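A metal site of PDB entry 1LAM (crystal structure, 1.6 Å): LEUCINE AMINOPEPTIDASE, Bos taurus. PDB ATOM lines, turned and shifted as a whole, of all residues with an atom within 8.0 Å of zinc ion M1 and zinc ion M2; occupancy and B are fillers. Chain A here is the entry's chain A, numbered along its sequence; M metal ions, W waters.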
ATOM      1  N   VAL A 219      20.910  29.109 -29.502  1.00  0.00           N
ATOM      2  CA  VAL A 219      19.605  29.132 -28.866  1.00  0.00           C
ATOM      3  C   VAL A 219      19.713  28.664 -27.413  1.00  0.00           C
ATOM      4  O   VAL A 219      19.198  29.314 -26.500  1.00  0.00           O
ATOM      5  CB  VAL A 219      18.620  28.207 -29.606  1.00  0.00           C
ATOM      6  CG1 VAL A 219      17.293  28.133 -28.860  1.00  0.00           C
ATOM      7  CG2 VAL A 219      18.401  28.709 -31.026  1.00  0.00           C
ATOM      8  N   LYS A 250      11.749  19.248 -33.516  1.00  0.00           N
ATOM      9  CA  LYS A 250      12.117  20.444 -32.753  1.00  0.00           C
ATOM     10  C   LYS A 250      11.819  20.182 -31.271  1.00  0.00           C
ATOM     11  O   LYS A 250      10.652  19.948 -30.901  1.00  0.00           O
ATOM     12  CB  LYS A 250      11.284  21.641 -33.240  1.00  0.00           C
ATOM     13  CG  LYS A 250      11.414  22.895 -32.372  1.00  0.00           C
ATOM     14  CD  LYS A 250      10.467  23.999 -32.835  1.00  0.00           C
ATOM     15  CE  LYS A 250      10.426  25.139 -31.806  1.00  0.00           C
ATOM     16  NZ  LYS A 250       9.504  26.251 -32.190  1.00  0.00           N
ATOM     17  N   GLY A 251      12.858  20.218 -30.440  1.00  0.00           N
ATOM     18  CA  GLY A 251      12.687  19.979 -29.009  1.00  0.00           C
ATOM     19  C   GLY A 251      12.938  21.151 -28.073  1.00  0.00           C
ATOM     20  O   GLY A 251      13.804  21.085 -27.187  1.00  0.00           O
ATOM     21  N   ILE A 252      12.218  22.253 -28.253  1.00  0.00           N
ATOM     22  CA  ILE A 252      12.369  23.400 -27.370  1.00  0.00           C
ATOM     23  C   ILE A 252      11.454  23.067 -26.174  1.00  0.00           C
ATOM     24  O   ILE A 252      10.228  23.138 -26.278  1.00  0.00           O
ATOM     25  CB  ILE A 252      11.943  24.708 -28.080  1.00  0.00           C
ATOM     26  CG1 ILE A 252      12.915  25.025 -29.234  1.00  0.00           C
ATOM     27  CG2 ILE A 252      11.903  25.873 -27.079  1.00  0.00           C
ATOM     28  CD1 ILE A 252      14.347  25.402 -28.792  1.00  0.00           C
ATOM     29  N   THR A 253      12.048  22.665 -25.050  1.00  0.00           N
ATOM     30  CA  THR A 253      11.269  22.268 -23.870  1.00  0.00           C
ATOM     31  C   THR A 253      10.439  23.402 -23.261  1.00  0.00           C
ATOM     32  O   THR A 253       9.432  23.160 -22.581  1.00  0.00           O
ATOM     33  CB  THR A 253      12.145  21.511 -22.841  1.00  0.00           C
ATOM     34  OG1 THR A 253      13.256  22.325 -22.455  1.00  0.00           O
ATOM     35  CG2 THR A 253      12.687  20.227 -23.466  1.00  0.00           C
ATOM     36  N   PHE A 254      10.913  24.631 -23.450  1.00  0.00           N
ATOM     37  CA  PHE A 254      10.175  25.834 -23.063  1.00  0.00           C
ATOM     38  C   PHE A 254      10.681  27.004 -23.898  1.00  0.00           C
ATOM     39  O   PHE A 254      11.893  27.229 -24.005  1.00  0.00           O
ATOM     40  CB  PHE A 254      10.204  26.232 -21.584  1.00  0.00           C
ATOM     41  CG  PHE A 254       9.236  27.369 -21.282  1.00  0.00           C
ATOM     42  CD1 PHE A 254       7.865  27.101 -21.204  1.00  0.00           C
ATOM     43  CD2 PHE A 254       9.664  28.695 -21.260  1.00  0.00           C
ATOM     44  CE1 PHE A 254       6.938  28.151 -21.094  1.00  0.00           C
ATOM     45  CE2 PHE A 254       8.745  29.740 -21.146  1.00  0.00           C
ATOM     46  CZ  PHE A 254       7.380  29.470 -21.081  1.00  0.00           C
ATOM     47  N   ASP A 255       9.735  27.719 -24.482  1.00  0.00           N
ATOM     48  CA  ASP A 255      10.047  28.865 -25.332  1.00  0.00           C
ATOM     49  C   ASP A 255       9.448  30.165 -24.749  1.00  0.00           C
ATOM     50  O   ASP A 255       8.222  30.370 -24.809  1.00  0.00           O
ATOM     51  CB  ASP A 255       9.493  28.607 -26.741  1.00  0.00           C
ATOM     52  CG  ASP A 255       9.930  29.644 -27.752  1.00  0.00           C
ATOM     53  OD1 ASP A 255      10.838  30.449 -27.442  1.00  0.00           O
ATOM     54  OD2 ASP A 255       9.350  29.647 -28.864  1.00  0.00           O
ATOM     55  N   SER A 256      10.303  31.021 -24.192  1.00  0.00           N
ATOM     56  CA  SER A 256       9.868  32.315 -23.663  1.00  0.00           C
ATOM     57  C   SER A 256       9.967  33.367 -24.780  1.00  0.00           C
ATOM     58  O   SER A 256       9.514  34.516 -24.630  1.00  0.00           O
ATOM     59  CB  SER A 256      10.788  32.772 -22.526  1.00  0.00           C
ATOM     60  OG  SER A 256      12.054  33.151 -23.052  1.00  0.00           O
ATOM     61  N   GLY A 257      10.602  32.963 -25.877  1.00  0.00           N
ATOM     62  CA  GLY A 257      10.822  33.839 -27.003  1.00  0.00           C
ATOM     63  C   GLY A 257      12.247  34.393 -26.957  1.00  0.00           C
ATOM     64  O   GLY A 257      12.805  34.758 -27.991  1.00  0.00           O
ATOM     65  N   GLY A 258      12.855  34.382 -25.762  1.00  0.00           N
ATOM     66  CA  GLY A 258      14.200  34.919 -25.583  1.00  0.00           C
ATOM     67  C   GLY A 258      14.147  36.432 -25.457  1.00  0.00           C
ATOM     68  O   GLY A 258      13.186  36.972 -24.907  1.00  0.00           O
ATOM     69  N   SER A 260      13.554  38.509 -27.741  1.00  0.00           N
ATOM     70  CA  SER A 260      12.355  38.892 -28.501  1.00  0.00           C
ATOM     71  C   SER A 260      11.249  38.187 -27.713  1.00  0.00           C
ATOM     72  O   SER A 260      10.526  37.323 -28.244  1.00  0.00           O
ATOM     73  CB  SER A 260      12.446  38.300 -29.909  1.00  0.00           C
ATOM     74  OG  SER A 260      13.574  38.782 -30.614  1.00  0.00           O
ATOM     75  N   LYS A 262       8.070  36.773 -25.547  1.00  0.00           N
ATOM     76  CA  LYS A 262       6.645  36.570 -25.823  1.00  0.00           C
ATOM     77  C   LYS A 262       5.740  37.338 -24.856  1.00  0.00           C
ATOM     78  O   LYS A 262       6.178  37.782 -23.796  1.00  0.00           O
ATOM     79  CB  LYS A 262       6.286  35.083 -25.715  1.00  0.00           C
ATOM     80  CG  LYS A 262       6.881  34.219 -26.788  1.00  0.00           C
ATOM     81  CD  LYS A 262       6.498  32.748 -26.545  1.00  0.00           C
ATOM     82  CE  LYS A 262       6.981  31.849 -27.659  1.00  0.00           C
ATOM     83  NZ  LYS A 262       6.384  32.228 -28.966  1.00  0.00           N
ATOM     84  N   MET A 270       3.695  27.038 -24.088  1.00  0.00           N
ATOM     85  CA  MET A 270       4.998  26.889 -24.732  1.00  0.00           C
ATOM     86  C   MET A 270       5.837  25.749 -24.128  1.00  0.00           C
ATOM     87  O   MET A 270       6.958  25.474 -24.584  1.00  0.00           O
ATOM     88  CB  MET A 270       5.754  28.218 -24.758  1.00  0.00           C
ATOM     89  CG  MET A 270       5.112  29.264 -25.666  1.00  0.00           C
ATOM     90  SD  MET A 270       4.978  28.658 -27.401  1.00  0.00           S
ATOM     91  CE  MET A 270       3.292  28.243 -27.474  1.00  0.00           C
ATOM     92  N   ALA A 272       4.958  23.025 -24.512  1.00  0.00           N
ATOM     93  CA  ALA A 272       4.752  22.042 -25.574  1.00  0.00           C
ATOM     94  C   ALA A 272       5.481  22.404 -26.863  1.00  0.00           C
ATOM     95  O   ALA A 272       5.186  21.820 -27.913  1.00  0.00           O
ATOM     96  CB  ALA A 272       3.257  21.836 -25.840  1.00  0.00           C
ATOM     97  N   ASP A 273       6.444  23.323 -26.778  1.00  0.00           N
ATOM     98  CA  ASP A 273       7.198  23.725 -27.977  1.00  0.00           C
ATOM     99  C   ASP A 273       8.179  22.609 -28.378  1.00  0.00           C
ATOM    100  O   ASP A 273       9.001  22.780 -29.279  1.00  0.00           O
ATOM    101  CB  ASP A 273       7.920  25.056 -27.745  1.00  0.00           C
ATOM    102  CG  ASP A 273       8.148  25.845 -29.046  1.00  0.00           C
ATOM    103  OD1 ASP A 273       7.364  25.727 -30.018  1.00  0.00           O
ATOM    104  OD2 ASP A 273       9.129  26.631 -29.085  1.00  0.00           O
ATOM    105  N   MET A 274       8.112  21.482 -27.662  1.00  0.00           N
ATOM    106  CA  MET A 274       8.924  20.316 -27.961  1.00  0.00           C
ATOM    107  C   MET A 274       8.014  19.235 -28.577  1.00  0.00           C
ATOM    108  O   MET A 274       8.401  18.062 -28.650  1.00  0.00           O
ATOM    109  CB  MET A 274       9.644  19.801 -26.693  1.00  0.00           C
ATOM    110  CG  MET A 274       8.848  19.922 -25.369  1.00  0.00           C
ATOM    111  SD  MET A 274       7.260  19.067 -25.349  1.00  0.00           S
ATOM    112  CE  MET A 274       7.796  17.356 -25.358  1.00  0.00           C
ATOM    113  N   ASN A 305      14.625  28.191 -24.535  1.00  0.00           N
ATOM    114  CA  ASN A 305      14.882  29.487 -25.172  1.00  0.00           C
ATOM    115  C   ASN A 305      14.497  30.495 -24.085  1.00  0.00           C
ATOM    116  O   ASN A 305      13.312  30.781 -23.877  1.00  0.00           O
ATOM    117  CB  ASN A 305      14.026  29.681 -26.445  1.00  0.00           C
ATOM    118  CG  ASN A 305      14.460  30.882 -27.277  1.00  0.00           C
ATOM    119  OD1 ASN A 305      15.615  31.315 -27.206  1.00  0.00           O
ATOM    120  ND2 ASN A 305      13.556  31.422 -28.075  1.00  0.00           N
ATOM    121  N   ASN A 330      15.047  37.769 -35.052  1.00  0.00           N
ATOM    122  CA  ASN A 330      14.040  37.587 -34.002  1.00  0.00           C
ATOM    123  C   ASN A 330      14.397  36.282 -33.275  1.00  0.00           C
ATOM    124  O   ASN A 330      14.389  35.210 -33.877  1.00  0.00           O
ATOM    125  CB  ASN A 330      12.644  37.526 -34.636  1.00  0.00           C
ATOM    126  CG  ASN A 330      11.549  37.463 -33.606  1.00  0.00           C
ATOM    127  OD1 ASN A 330      11.561  36.578 -32.763  1.00  0.00           O
ATOM    128  ND2 ASN A 330      10.629  38.417 -33.632  1.00  0.00           N
ATOM    129  N   THR A 331      14.755  36.384 -31.989  1.00  0.00           N
ATOM    130  CA  THR A 331      15.157  35.221 -31.199  1.00  0.00           C
ATOM    131  C   THR A 331      14.036  34.213 -30.913  1.00  0.00           C
ATOM    132  O   THR A 331      14.299  33.125 -30.376  1.00  0.00           O
ATOM    133  CB  THR A 331      15.836  35.632 -29.867  1.00  0.00           C
ATOM    134  OG1 THR A 331      14.865  36.254 -29.001  1.00  0.00           O
ATOM    135  CG2 THR A 331      16.970  36.632 -30.116  1.00  0.00           C
ATOM    136  N   ASP A 332      12.796  34.594 -31.215  1.00  0.00           N
ATOM    137  CA  ASP A 332      11.657  33.726 -31.010  1.00  0.00           C
ATOM    138  C   ASP A 332      11.474  32.809 -32.238  1.00  0.00           C
ATOM    139  O   ASP A 332      10.640  31.905 -32.216  1.00  0.00           O
ATOM    140  CB  ASP A 332      10.396  34.554 -30.711  1.00  0.00           C
ATOM    141  CG  ASP A 332       9.236  33.701 -30.143  1.00  0.00           C
ATOM    142  OD1 ASP A 332       9.421  32.493 -29.796  1.00  0.00           O
ATOM    143  OD2 ASP A 332       8.132  34.268 -30.033  1.00  0.00           O
ATOM    144  N   ALA A 333      12.225  33.055 -33.307  1.00  0.00           N
ATOM    145  CA  ALA A 333      12.175  32.186 -34.497  1.00  0.00           C
ATOM    146  C   ALA A 333      13.363  31.227 -34.294  1.00  0.00           C
ATOM    147  O   ALA A 333      14.277  31.140 -35.138  1.00  0.00           O
ATOM    148  CB  ALA A 333      12.333  33.004 -35.778  1.00  0.00           C
ATOM    149  N   GLU A 334      13.373  30.573 -33.136  1.00  0.00           N
ATOM    150  CA  GLU A 334      14.466  29.674 -32.736  1.00  0.00           C
ATOM    151  C   GLU A 334      14.361  28.223 -33.190  1.00  0.00           C
ATOM    152  O   GLU A 334      15.389  27.538 -33.326  1.00  0.00           O
ATOM    153  CB  GLU A 334      14.676  29.725 -31.199  1.00  0.00           C
ATOM    154  CG  GLU A 334      13.832  28.743 -30.363  1.00  0.00           C
ATOM    155  CD  GLU A 334      12.332  28.997 -30.424  1.00  0.00           C
ATOM    156  OE1 GLU A 334      11.915  30.181 -30.451  1.00  0.00           O
ATOM    157  OE2 GLU A 334      11.549  28.011 -30.420  1.00  0.00           O
ATOM    158  N   GLY A 335      13.139  27.759 -33.432  1.00  0.00           N
ATOM    159  CA  GLY A 335      12.963  26.386 -33.861  1.00  0.00           C
ATOM    160  C   GLY A 335      13.705  26.124 -35.158  1.00  0.00           C
ATOM    161  O   GLY A 335      14.400  25.094 -35.283  1.00  0.00           O
ATOM    162  N   ARG A 336      13.607  27.058 -36.095  1.00  0.00           N
ATOM    163  CA  ARG A 336      14.275  26.900 -37.380  1.00  0.00           C
ATOM    164  C   ARG A 336      15.798  26.918 -37.222  1.00  0.00           C
ATOM    165  O   ARG A 336      16.528  26.260 -37.980  1.00  0.00           O
ATOM    166  CB  ARG A 336      13.764  27.921 -38.422  1.00  0.00           C
ATOM    167  CG  ARG A 336      14.146  29.376 -38.179  1.00  0.00           C
ATOM    168  CD  ARG A 336      13.256  30.302 -39.005  1.00  0.00           C
ATOM    169  NE  ARG A 336      11.920  30.439 -38.404  1.00  0.00           N
ATOM    170  CZ  ARG A 336      10.945  31.221 -38.864  1.00  0.00           C
ATOM    171  NH1 ARG A 336      11.105  31.943 -39.963  1.00  0.00           N
ATOM    172  NH2 ARG A 336       9.776  31.267 -38.222  1.00  0.00           N
ATOM    173  N   ILE A 338      17.595  25.621 -34.522  1.00  0.00           N
ATOM    174  CA  ILE A 338      18.037  24.313 -34.054  1.00  0.00           C
ATOM    175  C   ILE A 338      17.791  23.223 -35.128  1.00  0.00           C
ATOM    176  O   ILE A 338      18.572  22.259 -35.230  1.00  0.00           O
ATOM    177  CB  ILE A 338      17.404  23.904 -32.662  1.00  0.00           C
ATOM    178  CG1 ILE A 338      15.969  23.390 -32.813  1.00  0.00           C
ATOM    179  CG2 ILE A 338      17.459  25.106 -31.682  1.00  0.00           C
ATOM    180  CD1 ILE A 338      15.372  22.884 -31.496  1.00  0.00           C
ATOM    181  N   ALA A 358       7.597  20.051 -36.246  1.00  0.00           N
ATOM    182  CA  ALA A 358       7.863  21.177 -35.365  1.00  0.00           C
ATOM    183  C   ALA A 358       6.633  22.038 -35.091  1.00  0.00           C
ATOM    184  O   ALA A 358       5.828  22.264 -35.998  1.00  0.00           O
ATOM    185  CB  ALA A 358       8.942  22.059 -35.988  1.00  0.00           C
ATOM    186  N   THR A 359       6.502  22.513 -33.849  1.00  0.00           N
ATOM    187  CA  THR A 359       5.420  23.434 -33.461  1.00  0.00           C
ATOM    188  C   THR A 359       6.126  24.723 -33.860  1.00  0.00           C
ATOM    189  O   THR A 359       6.575  25.505 -33.016  1.00  0.00           O
ATOM    190  CB  THR A 359       5.169  23.395 -31.931  1.00  0.00           C
ATOM    191  OG1 THR A 359       6.403  23.459 -31.226  1.00  0.00           O
ATOM    192  CG2 THR A 359       4.429  22.124 -31.519  1.00  0.00           C
ATOM    193  N   LEU A 360       6.215  24.954 -35.169  1.00  0.00           N
ATOM    194  CA  LEU A 360       6.977  26.081 -35.676  1.00  0.00           C
ATOM    195  C   LEU A 360       6.439  27.498 -35.730  1.00  0.00           C
ATOM    196  O   LEU A 360       7.119  28.426 -35.267  1.00  0.00           O
ATOM    197  CB  LEU A 360       7.611  25.694 -37.018  1.00  0.00           C
ATOM    198  CG  LEU A 360       8.941  26.371 -37.402  1.00  0.00           C
ATOM    199  CD1 LEU A 360      10.061  25.967 -36.445  1.00  0.00           C
ATOM    200  CD2 LEU A 360       9.318  26.004 -38.833  1.00  0.00           C
ATOM    201  N   THR A 361       5.229  27.711 -36.267  1.00  0.00           N
ATOM    202  CA  THR A 361       4.761  29.086 -36.400  1.00  0.00           C
ATOM    203  C   THR A 361       3.333  29.374 -35.991  1.00  0.00           C
ATOM    204  O   THR A 361       2.436  28.544 -36.182  1.00  0.00           O
ATOM    205  CB  THR A 361       4.912  29.586 -37.881  1.00  0.00           C
ATOM    206  OG1 THR A 361       4.016  28.850 -38.736  1.00  0.00           O
ATOM    207  CG2 THR A 361       6.356  29.413 -38.390  1.00  0.00           C
HETATM  208 ZN    ZN M   1       9.561  27.770 -30.646  1.00  0.00          ZN
HETATM  209 ZN    ZN M   2       9.978  30.758 -30.563  1.00  0.00          ZN
HETATM  210  O   HOH W   1       8.990  29.357 -31.627  1.00  0.00           O
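Zinc ion M2 is bound by OD1 of Asp 332, water W1, OE1 of Glu 334, O of Asp 332 and OD2 of Asp 255.
The backbone NH (N) of Asp 332 is in hydrogen-bond range of the side-chain amide oxygen (OD1) of Asn 330, at 2.8 Å. O of Asp 273 is in hydrogen-bond range of N of Ile 252. NZ of Lys 262 lies within salt-bridge range of OD2 of Asp 332 (2.9 Å). The backbone NH of Asp 332 lies within hydrogen-bond range of the backbone carbonyl oxygen of Gly 257, 3.2 Å away. OD1 of Asp 255 is in hydrogen-bond range of ND2 of Asn 305, at 3.0 Å. O of Thr 359 lies close to NZ of Lys 250, at 3.1 Å. OE1 of Glu 334 lies close to ND2 of Asn 305 (3.1 Å). OD1 of Asp 255 is in hydrogen-bond range of N of Gly 257 (3.0 Å).
Of the 29 residues printed, 3 come within 4 Å of zinc ion M2. The nearest printed residue that does not touch zinc ion M2 is Lys 262 (4.2 Å).
Water W1 is bound to zinc ion M1, 2.0 Å away. Zinc ion M1 is bound by OD2 of Asp 273, 2.0 Å away. Zinc ion M1 is bound by the side-chain carboxylate (OE2) of Glu 334 (2.0 Å). Zinc ion M1 is bound by NZ of Lys 250. The side-chain carboxylate (OD2) of Asp 255 binds zinc ion M1 (2.6 Å).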
